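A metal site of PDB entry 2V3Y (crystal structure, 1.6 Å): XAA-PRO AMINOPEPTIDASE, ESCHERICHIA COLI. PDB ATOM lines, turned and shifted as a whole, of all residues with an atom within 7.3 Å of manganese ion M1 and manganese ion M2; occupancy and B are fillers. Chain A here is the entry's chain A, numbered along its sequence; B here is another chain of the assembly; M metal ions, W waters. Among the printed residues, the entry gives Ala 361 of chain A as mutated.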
ATOM      1  N   TYR A 229     -15.635  11.605   8.307  1.00  0.00           N
ATOM      2  CA  TYR A 229     -16.938  12.271   8.281  1.00  0.00           C
ATOM      3  C   TYR A 229     -16.818  13.556   9.092  1.00  0.00           C
ATOM      4  O   TYR A 229     -15.851  13.720   9.835  1.00  0.00           O
ATOM      5  CB  TYR A 229     -18.048  11.409   8.832  1.00  0.00           C
ATOM      6  CG  TYR A 229     -17.788  10.922  10.226  1.00  0.00           C
ATOM      7  CD1 TYR A 229     -17.031   9.750  10.436  1.00  0.00           C
ATOM      8  CD2 TYR A 229     -18.252  11.594  11.337  1.00  0.00           C
ATOM      9  CE1 TYR A 229     -16.732   9.298  11.704  1.00  0.00           C
ATOM     10  CE2 TYR A 229     -17.995  11.130  12.632  1.00  0.00           C
ATOM     11  CZ  TYR A 229     -17.213   9.970  12.830  1.00  0.00           C
ATOM     12  OH  TYR A 229     -16.917   9.497  14.087  1.00  0.00           O
ATOM     13  N   ILE A 232     -18.511  15.847  15.040  1.00  0.00           N
ATOM     14  CA  ILE A 232     -19.650  16.275  15.850  1.00  0.00           C
ATOM     15  C   ILE A 232     -19.130  16.563  17.259  1.00  0.00           C
ATOM     16  O   ILE A 232     -18.551  15.663  17.875  1.00  0.00           O
ATOM     17  CB  ILE A 232     -20.690  15.117  15.895  1.00  0.00           C
ATOM     18  CG1 ILE A 232     -21.335  14.942  14.518  1.00  0.00           C
ATOM     19  CG2 ILE A 232     -21.722  15.331  16.995  1.00  0.00           C
ATOM     20  CD1 ILE A 232     -21.810  13.518  14.223  1.00  0.00           C
ATOM     21  N   ILE A 259     -18.800  13.787  21.609  1.00  0.00           N
ATOM     22  CA  ILE A 259     -17.891  13.904  20.481  1.00  0.00           C
ATOM     23  C   ILE A 259     -18.001  12.638  19.641  1.00  0.00           C
ATOM     24  O   ILE A 259     -17.688  11.567  20.128  1.00  0.00           O
ATOM     25  CB  ILE A 259     -16.421  14.139  20.892  1.00  0.00           C
ATOM     26  CG1 ILE A 259     -16.322  15.405  21.760  1.00  0.00           C
ATOM     27  CG2 ILE A 259     -15.535  14.227  19.647  1.00  0.00           C
ATOM     28  CD1 ILE A 259     -14.895  15.784  22.106  1.00  0.00           C
ATOM     29  N   ASP A 260     -18.425  12.789  18.382  1.00  0.00           N
ATOM     30  CA  ASP A 260     -18.475  11.681  17.412  1.00  0.00           C
ATOM     31  C   ASP A 260     -17.507  12.095  16.301  1.00  0.00           C
ATOM     32  O   ASP A 260     -17.738  13.090  15.613  1.00  0.00           O
ATOM     33  CB  ASP A 260     -19.910  11.493  16.906  1.00  0.00           C
ATOM     34  CG  ASP A 260     -20.131  10.163  16.162  1.00  0.00           C
ATOM     35  OD1 ASP A 260     -19.151   9.620  15.657  1.00  0.00           O
ATOM     36  OD2 ASP A 260     -21.293   9.743  16.104  1.00  0.00           O
ATOM     37  N   ALA A 261     -16.349  11.443  16.255  1.00  0.00           N
ATOM     38  CA  ALA A 261     -15.283  11.795  15.318  1.00  0.00           C
ATOM     39  C   ALA A 261     -14.480  10.583  14.962  1.00  0.00           C
ATOM     40  O   ALA A 261     -14.302   9.670  15.756  1.00  0.00           O
ATOM     41  CB  ALA A 261     -14.329  12.874  15.912  1.00  0.00           C
ATOM     42  N   GLY A 262     -14.030  10.554  13.719  1.00  0.00           N
ATOM     43  CA  GLY A 262     -13.251   9.422  13.220  1.00  0.00           C
ATOM     44  C   GLY A 262     -12.309   9.823  12.099  1.00  0.00           C
ATOM     45  O   GLY A 262     -12.611  10.748  11.339  1.00  0.00           O
ATOM     46  N   GLY A 270     -12.173   5.182  10.961  1.00  0.00           N
ATOM     47  CA  GLY A 270     -12.498   5.069  12.358  1.00  0.00           C
ATOM     48  C   GLY A 270     -13.812   5.794  12.652  1.00  0.00           C
ATOM     49  O   GLY A 270     -14.228   6.700  11.909  1.00  0.00           O
ATOM     50  N   ASP A 271     -14.440   5.479  13.784  1.00  0.00           N
ATOM     51  CA  ASP A 271     -15.732   6.067  14.112  1.00  0.00           C
ATOM     52  C   ASP A 271     -15.988   5.823  15.585  1.00  0.00           C
ATOM     53  O   ASP A 271     -16.511   4.779  15.977  1.00  0.00           O
ATOM     54  CB  ASP A 271     -16.826   5.463  13.240  1.00  0.00           C
ATOM     55  CG  ASP A 271     -18.195   5.993  13.559  1.00  0.00           C
ATOM     56  OD1 ASP A 271     -18.320   6.956  14.361  1.00  0.00           O
ATOM     57  OD2 ASP A 271     -19.169   5.476  12.974  1.00  0.00           O
ATOM     58  N   ILE A 272     -15.610   6.808  16.405  1.00  0.00           N
ATOM     59  CA  ILE A 272     -15.765   6.742  17.851  1.00  0.00           C
ATOM     60  C   ILE A 272     -16.659   7.845  18.345  1.00  0.00           C
ATOM     61  O   ILE A 272     -16.594   8.987  17.876  1.00  0.00           O
ATOM     62  CB  ILE A 272     -14.400   6.818  18.602  1.00  0.00           C
ATOM     63  CG1 ILE A 272     -13.520   5.602  18.245  1.00  0.00           C
ATOM     64  CG2 ILE A 272     -14.579   6.928  20.163  1.00  0.00           C
ATOM     65  CD1 ILE A 272     -12.154   5.636  18.954  1.00  0.00           C
ATOM     66  N   THR A 273     -17.502   7.503  19.322  1.00  0.00           N
ATOM     67  CA  THR A 273     -18.194   8.519  20.111  1.00  0.00           C
ATOM     68  C   THR A 273     -17.840   8.346  21.591  1.00  0.00           C
ATOM     69  O   THR A 273     -17.869   7.220  22.129  1.00  0.00           O
ATOM     70  CB  THR A 273     -19.721   8.514  19.931  1.00  0.00           C
ATOM     71  OG1 THR A 273     -20.073   8.491  18.522  1.00  0.00           O
ATOM     72  CG2 THR A 273     -20.366   9.770  20.625  1.00  0.00           C
ATOM     73  N   LEU A 352     -28.307   0.628  16.460  1.00  0.00           N
ATOM     74  CA  LEU A 352     -27.194   0.300  17.343  1.00  0.00           C
ATOM     75  C   LEU A 352     -25.855   0.194  16.598  1.00  0.00           C
ATOM     76  O   LEU A 352     -24.790   0.445  17.163  1.00  0.00           O
ATOM     77  CB  LEU A 352     -27.440  -1.057  18.012  1.00  0.00           C
ATOM     78  CG  LEU A 352     -26.395  -1.544  19.021  1.00  0.00           C
ATOM     79  CD1 LEU A 352     -26.336  -0.592  20.217  1.00  0.00           C
ATOM     80  CD2 LEU A 352     -26.737  -2.952  19.467  1.00  0.00           C
ATOM     81  N   SER A 353     -25.911  -0.219  15.336  1.00  0.00           N
ATOM     82  CA  SER A 353     -24.711  -0.607  14.605  1.00  0.00           C
ATOM     83  C   SER A 353     -24.807  -0.363  13.113  1.00  0.00           C
ATOM     84  O   SER A 353     -25.846  -0.585  12.504  1.00  0.00           O
ATOM     85  CB  SER A 353     -24.460  -2.112  14.804  1.00  0.00           C
ATOM     86  OG  SER A 353     -24.157  -2.428  16.158  1.00  0.00           O
ATOM     87  N   HIS A 354     -23.696   0.044  12.520  1.00  0.00           N
ATOM     88  CA  HIS A 354     -23.576   0.047  11.071  1.00  0.00           C
ATOM     89  C   HIS A 354     -22.237  -0.571  10.688  1.00  0.00           C
ATOM     90  O   HIS A 354     -21.262  -0.546  11.448  1.00  0.00           O
ATOM     91  CB  HIS A 354     -23.703   1.469  10.492  1.00  0.00           C
ATOM     92  CG  HIS A 354     -22.709   2.457  11.040  1.00  0.00           C
ATOM     93  ND1 HIS A 354     -21.425   2.573  10.550  1.00  0.00           N
ATOM     94  CD2 HIS A 354     -22.803   3.365  12.042  1.00  0.00           C
ATOM     95  CE1 HIS A 354     -20.774   3.511  11.225  1.00  0.00           C
ATOM     96  NE2 HIS A 354     -21.577   3.994  12.154  1.00  0.00           N
ATOM     97  N   TRP A 355     -22.180  -1.122   9.477  1.00  0.00           N
ATOM     98  CA  TRP A 355     -20.913  -1.595   8.918  1.00  0.00           C
ATOM     99  C   TRP A 355     -19.902  -0.481   8.851  1.00  0.00           C
ATOM    100  O   TRP A 355     -20.287   0.694   8.690  1.00  0.00           O
ATOM    101  CB  TRP A 355     -21.110  -2.118   7.501  1.00  0.00           C
ATOM    102  CG  TRP A 355     -22.200  -3.135   7.293  1.00  0.00           C
ATOM    103  CD1 TRP A 355     -23.142  -3.080   6.305  1.00  0.00           C
ATOM    104  CD2 TRP A 355     -22.412  -4.387   7.984  1.00  0.00           C
ATOM    105  NE1 TRP A 355     -23.948  -4.188   6.351  1.00  0.00           N
ATOM    106  CE2 TRP A 355     -23.541  -5.008   7.380  1.00  0.00           C
ATOM    107  CE3 TRP A 355     -21.801  -5.015   9.075  1.00  0.00           C
ATOM    108  CZ2 TRP A 355     -24.045  -6.260   7.807  1.00  0.00           C
ATOM    109  CZ3 TRP A 355     -22.319  -6.257   9.506  1.00  0.00           C
ATOM    110  CH2 TRP A 355     -23.425  -6.859   8.868  1.00  0.00           C
ATOM    111  N   LEU A 356     -18.606  -0.836   8.866  1.00  0.00           N
ATOM    112  CA  LEU A 356     -17.509   0.147   8.860  1.00  0.00           C
ATOM    113  C   LEU A 356     -16.436  -0.298   7.849  1.00  0.00           C
ATOM    114  O   LEU A 356     -16.103  -1.500   7.804  1.00  0.00           O
ATOM    115  CB  LEU A 356     -16.914   0.280  10.261  1.00  0.00           C
ATOM    116  CG  LEU A 356     -15.849   1.339  10.544  1.00  0.00           C
ATOM    117  CD1 LEU A 356     -16.462   2.753  10.476  1.00  0.00           C
ATOM    118  CD2 LEU A 356     -15.210   1.074  11.941  1.00  0.00           C
ATOM    119  N   VAL A 360     -17.661   5.261   6.188  1.00  0.00           N
ATOM    120  CA  VAL A 360     -17.985   5.149   7.607  1.00  0.00           C
ATOM    121  C   VAL A 360     -19.291   4.421   7.811  1.00  0.00           C
ATOM    122  O   VAL A 360     -19.359   3.521   8.641  1.00  0.00           O
ATOM    123  CB  VAL A 360     -17.942   6.504   8.351  1.00  0.00           C
ATOM    124  CG1 VAL A 360     -18.924   7.496   7.789  1.00  0.00           C
ATOM    125  CG2 VAL A 360     -18.147   6.256   9.857  1.00  0.00           C
ATOM    126  N   ALA A 361     -20.306   4.774   7.024  1.00  0.00           N
ATOM    127  CA  ALA A 361     -21.552   3.985   6.972  1.00  0.00           C
ATOM    128  C   ALA A 361     -21.337   3.036   5.773  1.00  0.00           C
ATOM    129  O   ALA A 361     -21.662   3.342   4.628  1.00  0.00           O
ATOM    130  CB  ALA A 361     -22.800   4.869   6.811  1.00  0.00           C
ATOM    131  N   THR A 381     -19.864  -0.855  13.929  1.00  0.00           N
ATOM    132  CA  THR A 381     -19.870  -0.039  15.133  1.00  0.00           C
ATOM    133  C   THR A 381     -20.903  -0.526  16.130  1.00  0.00           C
ATOM    134  O   THR A 381     -21.798  -1.311  15.815  1.00  0.00           O
ATOM    135  CB  THR A 381     -20.196   1.381  14.795  1.00  0.00           C
ATOM    136  OG1 THR A 381     -21.570   1.475  14.384  1.00  0.00           O
ATOM    137  CG2 THR A 381     -19.195   1.920  13.706  1.00  0.00           C
ATOM    138  N   VAL A 382     -20.755  -0.047  17.365  1.00  0.00           N
ATOM    139  CA  VAL A 382     -21.712  -0.352  18.445  1.00  0.00           C
ATOM    140  C   VAL A 382     -21.897   1.002  19.136  1.00  0.00           C
ATOM    141  O   VAL A 382     -20.943   1.518  19.744  1.00  0.00           O
ATOM    142  CB  VAL A 382     -21.173  -1.404  19.428  1.00  0.00           C
ATOM    143  CG1 VAL A 382     -22.255  -1.845  20.426  1.00  0.00           C
ATOM    144  CG2 VAL A 382     -20.606  -2.601  18.646  1.00  0.00           C
ATOM    145  N   GLU A 383     -23.081   1.589  18.977  1.00  0.00           N
ATOM    146  CA  GLU A 383     -23.296   2.990  19.339  1.00  0.00           C
ATOM    147  C   GLU A 383     -24.651   3.260  19.975  1.00  0.00           C
ATOM    148  O   GLU A 383     -25.426   4.082  19.484  1.00  0.00           O
ATOM    149  CB  GLU A 383     -23.043   3.914  18.141  1.00  0.00           C
ATOM    150  CG  GLU A 383     -23.868   3.712  16.916  1.00  0.00           C
ATOM    151  CD  GLU A 383     -23.371   4.641  15.810  1.00  0.00           C
ATOM    152  OE1 GLU A 383     -23.358   5.889  15.979  1.00  0.00           O
ATOM    153  OE2 GLU A 383     -22.918   4.074  14.800  1.00  0.00           O
ATOM    154  N   ARG A 404     -23.981   9.407  23.838  1.00  0.00           N
ATOM    155  CA  ARG A 404     -23.722   8.280  22.966  1.00  0.00           C
ATOM    156  C   ARG A 404     -22.308   7.800  23.252  1.00  0.00           C
ATOM    157  O   ARG A 404     -21.421   8.593  23.532  1.00  0.00           O
ATOM    158  CB  ARG A 404     -23.861   8.682  21.485  1.00  0.00           C
ATOM    159  CG  ARG A 404     -23.563   7.541  20.499  1.00  0.00           C
ATOM    160  CD  ARG A 404     -24.049   7.828  19.069  1.00  0.00           C
ATOM    161  NE  ARG A 404     -23.433   8.983  18.399  1.00  0.00           N
ATOM    162  CZ  ARG A 404     -24.004  10.183  18.235  1.00  0.00           C
ATOM    163  NH1 ARG A 404     -25.183  10.470  18.760  1.00  0.00           N
ATOM    164  NH2 ARG A 404     -23.378  11.137  17.541  1.00  0.00           N
ATOM    165  N   GLU A 406     -19.605   4.954  21.571  1.00  0.00           N
ATOM    166  CA  GLU A 406     -19.462   4.120  20.381  1.00  0.00           C
ATOM    167  C   GLU A 406     -18.049   3.584  20.244  1.00  0.00           C
ATOM    168  O   GLU A 406     -17.076   4.350  20.301  1.00  0.00           O
ATOM    169  CB  GLU A 406     -19.828   4.941  19.151  1.00  0.00           C
ATOM    170  CG  GLU A 406     -19.447   4.328  17.808  1.00  0.00           C
ATOM    171  CD  GLU A 406     -19.897   5.186  16.639  1.00  0.00           C
ATOM    172  OE1 GLU A 406     -19.965   6.414  16.774  1.00  0.00           O
ATOM    173  OE2 GLU A 406     -20.177   4.597  15.590  1.00  0.00           O
ATOM    174  N   ASP A 407     -17.981   2.258  20.004  1.00  0.00           N
ATOM    175  CA  ASP A 407     -16.748   1.554  19.664  1.00  0.00           C
ATOM    176  C   ASP A 407     -16.897   0.895  18.270  1.00  0.00           C
ATOM    177  O   ASP A 407     -18.025   0.704  17.786  1.00  0.00           O
ATOM    178  CB  ASP A 407     -16.433   0.466  20.695  1.00  0.00           C
ATOM    179  CG  ASP A 407     -15.749   1.010  21.960  1.00  0.00           C
ATOM    180  OD1 ASP A 407     -15.098   2.103  21.871  1.00  0.00           O
ATOM    181  OD2 ASP A 407     -15.880   0.349  23.008  1.00  0.00           O
ATOM    182  N   ASP A 408     -15.752   0.571  17.678  1.00  0.00           N
ATOM    183  CA  ASP A 408     -15.660  -0.142  16.399  1.00  0.00           C
ATOM    184  C   ASP A 408     -15.127  -1.537  16.704  1.00  0.00           C
ATOM    185  O   ASP A 408     -14.124  -1.684  17.416  1.00  0.00           O
ATOM    186  CB  ASP A 408     -14.699   0.562  15.441  1.00  0.00           C
ATOM    187  CG  ASP A 408     -15.058   2.009  15.252  1.00  0.00           C
ATOM    188  OD1 ASP A 408     -16.276   2.339  15.368  1.00  0.00           O
ATOM    189  OD2 ASP A 408     -14.115   2.817  15.033  1.00  0.00           O
ATOM    190  N   PRO B   2     -24.703   8.332  13.477  1.00  0.00           N
ATOM    191  CA  PRO B   2     -25.607   7.185  13.689  1.00  0.00           C
ATOM    192  C   PRO B   2     -26.446   6.861  12.450  1.00  0.00           C
ATOM    193  O   PRO B   2     -26.758   7.773  11.664  1.00  0.00           O
ATOM    194  CB  PRO B   2     -26.517   7.662  14.822  1.00  0.00           C
ATOM    195  CG  PRO B   2     -25.701   8.688  15.576  1.00  0.00           C
ATOM    196  CD  PRO B   2     -24.669   9.239  14.642  1.00  0.00           C
ATOM    197  N   LEU B   3     -26.794   5.586  12.281  1.00  0.00           N
ATOM    198  CA  LEU B   3     -27.637   5.168  11.152  1.00  0.00           C
ATOM    199  C   LEU B   3     -29.093   4.976  11.604  1.00  0.00           C
ATOM    200  O   LEU B   3     -30.031   5.225  10.842  1.00  0.00           O
ATOM    201  CB  LEU B   3     -27.126   3.874  10.500  1.00  0.00           C
ATOM    202  CG  LEU B   3     -26.574   3.872   9.061  1.00  0.00           C
ATOM    203  CD1 LEU B   3     -26.633   2.455   8.475  1.00  0.00           C
ATOM    204  CD2 LEU B   3     -27.278   4.854   8.129  1.00  0.00           C
ATOM    205  OXT LEU B   3     -29.375   4.567  12.712  1.00  0.00           O
HETATM  206 MN    MN M   1     -20.041   7.666  15.134  1.00  0.00          MN
HETATM  207 MN    MN M   2     -21.092   5.189  13.807  1.00  0.00          MN
HETATM  208  O   HOH W   1     -21.474   7.117  14.302  1.00  0.00           O
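Thr 381 touches manganese ion M2 (CG2 to MN, 3.8 Å).
Five residues have an atom within 4 Å of manganese ion M2: Asp 271, His 354, Thr 381, Glu 383 and Glu 406.
OH of Tyr 229 lies close to OD1 of Asp 271 (2.9 Å).
The backbone NH of Thr 381 sits at hydrogen-bond distance from the backbone carbonyl oxygen of His 354 (2.9 Å).
O of Val 360 lies close to ND1 of His 354.
OE2 of Glu 383 lies close to OG1 of Thr 381, at 3.0 Å.
NE of Arg 404 lies within salt-bridge range of OE1 of Glu 383, 3.9 Å away.
The side-chain hydroxyl of Thr 273 sits at hydrogen-bond distance from the guanidinium group of Arg 404 (3.4 Å).
OH of Tyr 229 lies close to N of Ala 261.
OH of Tyr 229 is in hydrogen-bond range of N of Gly 262 (3.1 Å).
Merely in contact with manganese ion M1: Thr 273 and Tyr 229.
Of the 26 residues printed, 6 come within 4 Å of manganese ion M1.
Along chain A the residues within 4 Å of manganese ion M1 span positions 229 to 406.
The nearest printed residue that does not touch manganese ion M1 is Ile 272 (4.6 Å).
Manganese ion M1 is bound by water W1 (1.7 Å), the side-chain carboxylate (OD1) of Asp 271 (2.0 Å), the side-chain carboxylate (OE1) of Glu 406 (2.1 Å), the side-chain carboxylate (OD1) of Asp 260 (2.2 Å) and the side-chain carboxylate (OD2) of Asp 260 (2.6 Å).
Manganese ion M2 is bound by water W1 (2.0 Å), OE2 of Glu 406 (2.1 Å), NE2 of His 354 (2.1 Å), OD2 of Asp 271 (2.1 Å) and OE2 of Glu 383 (2.4 Å).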
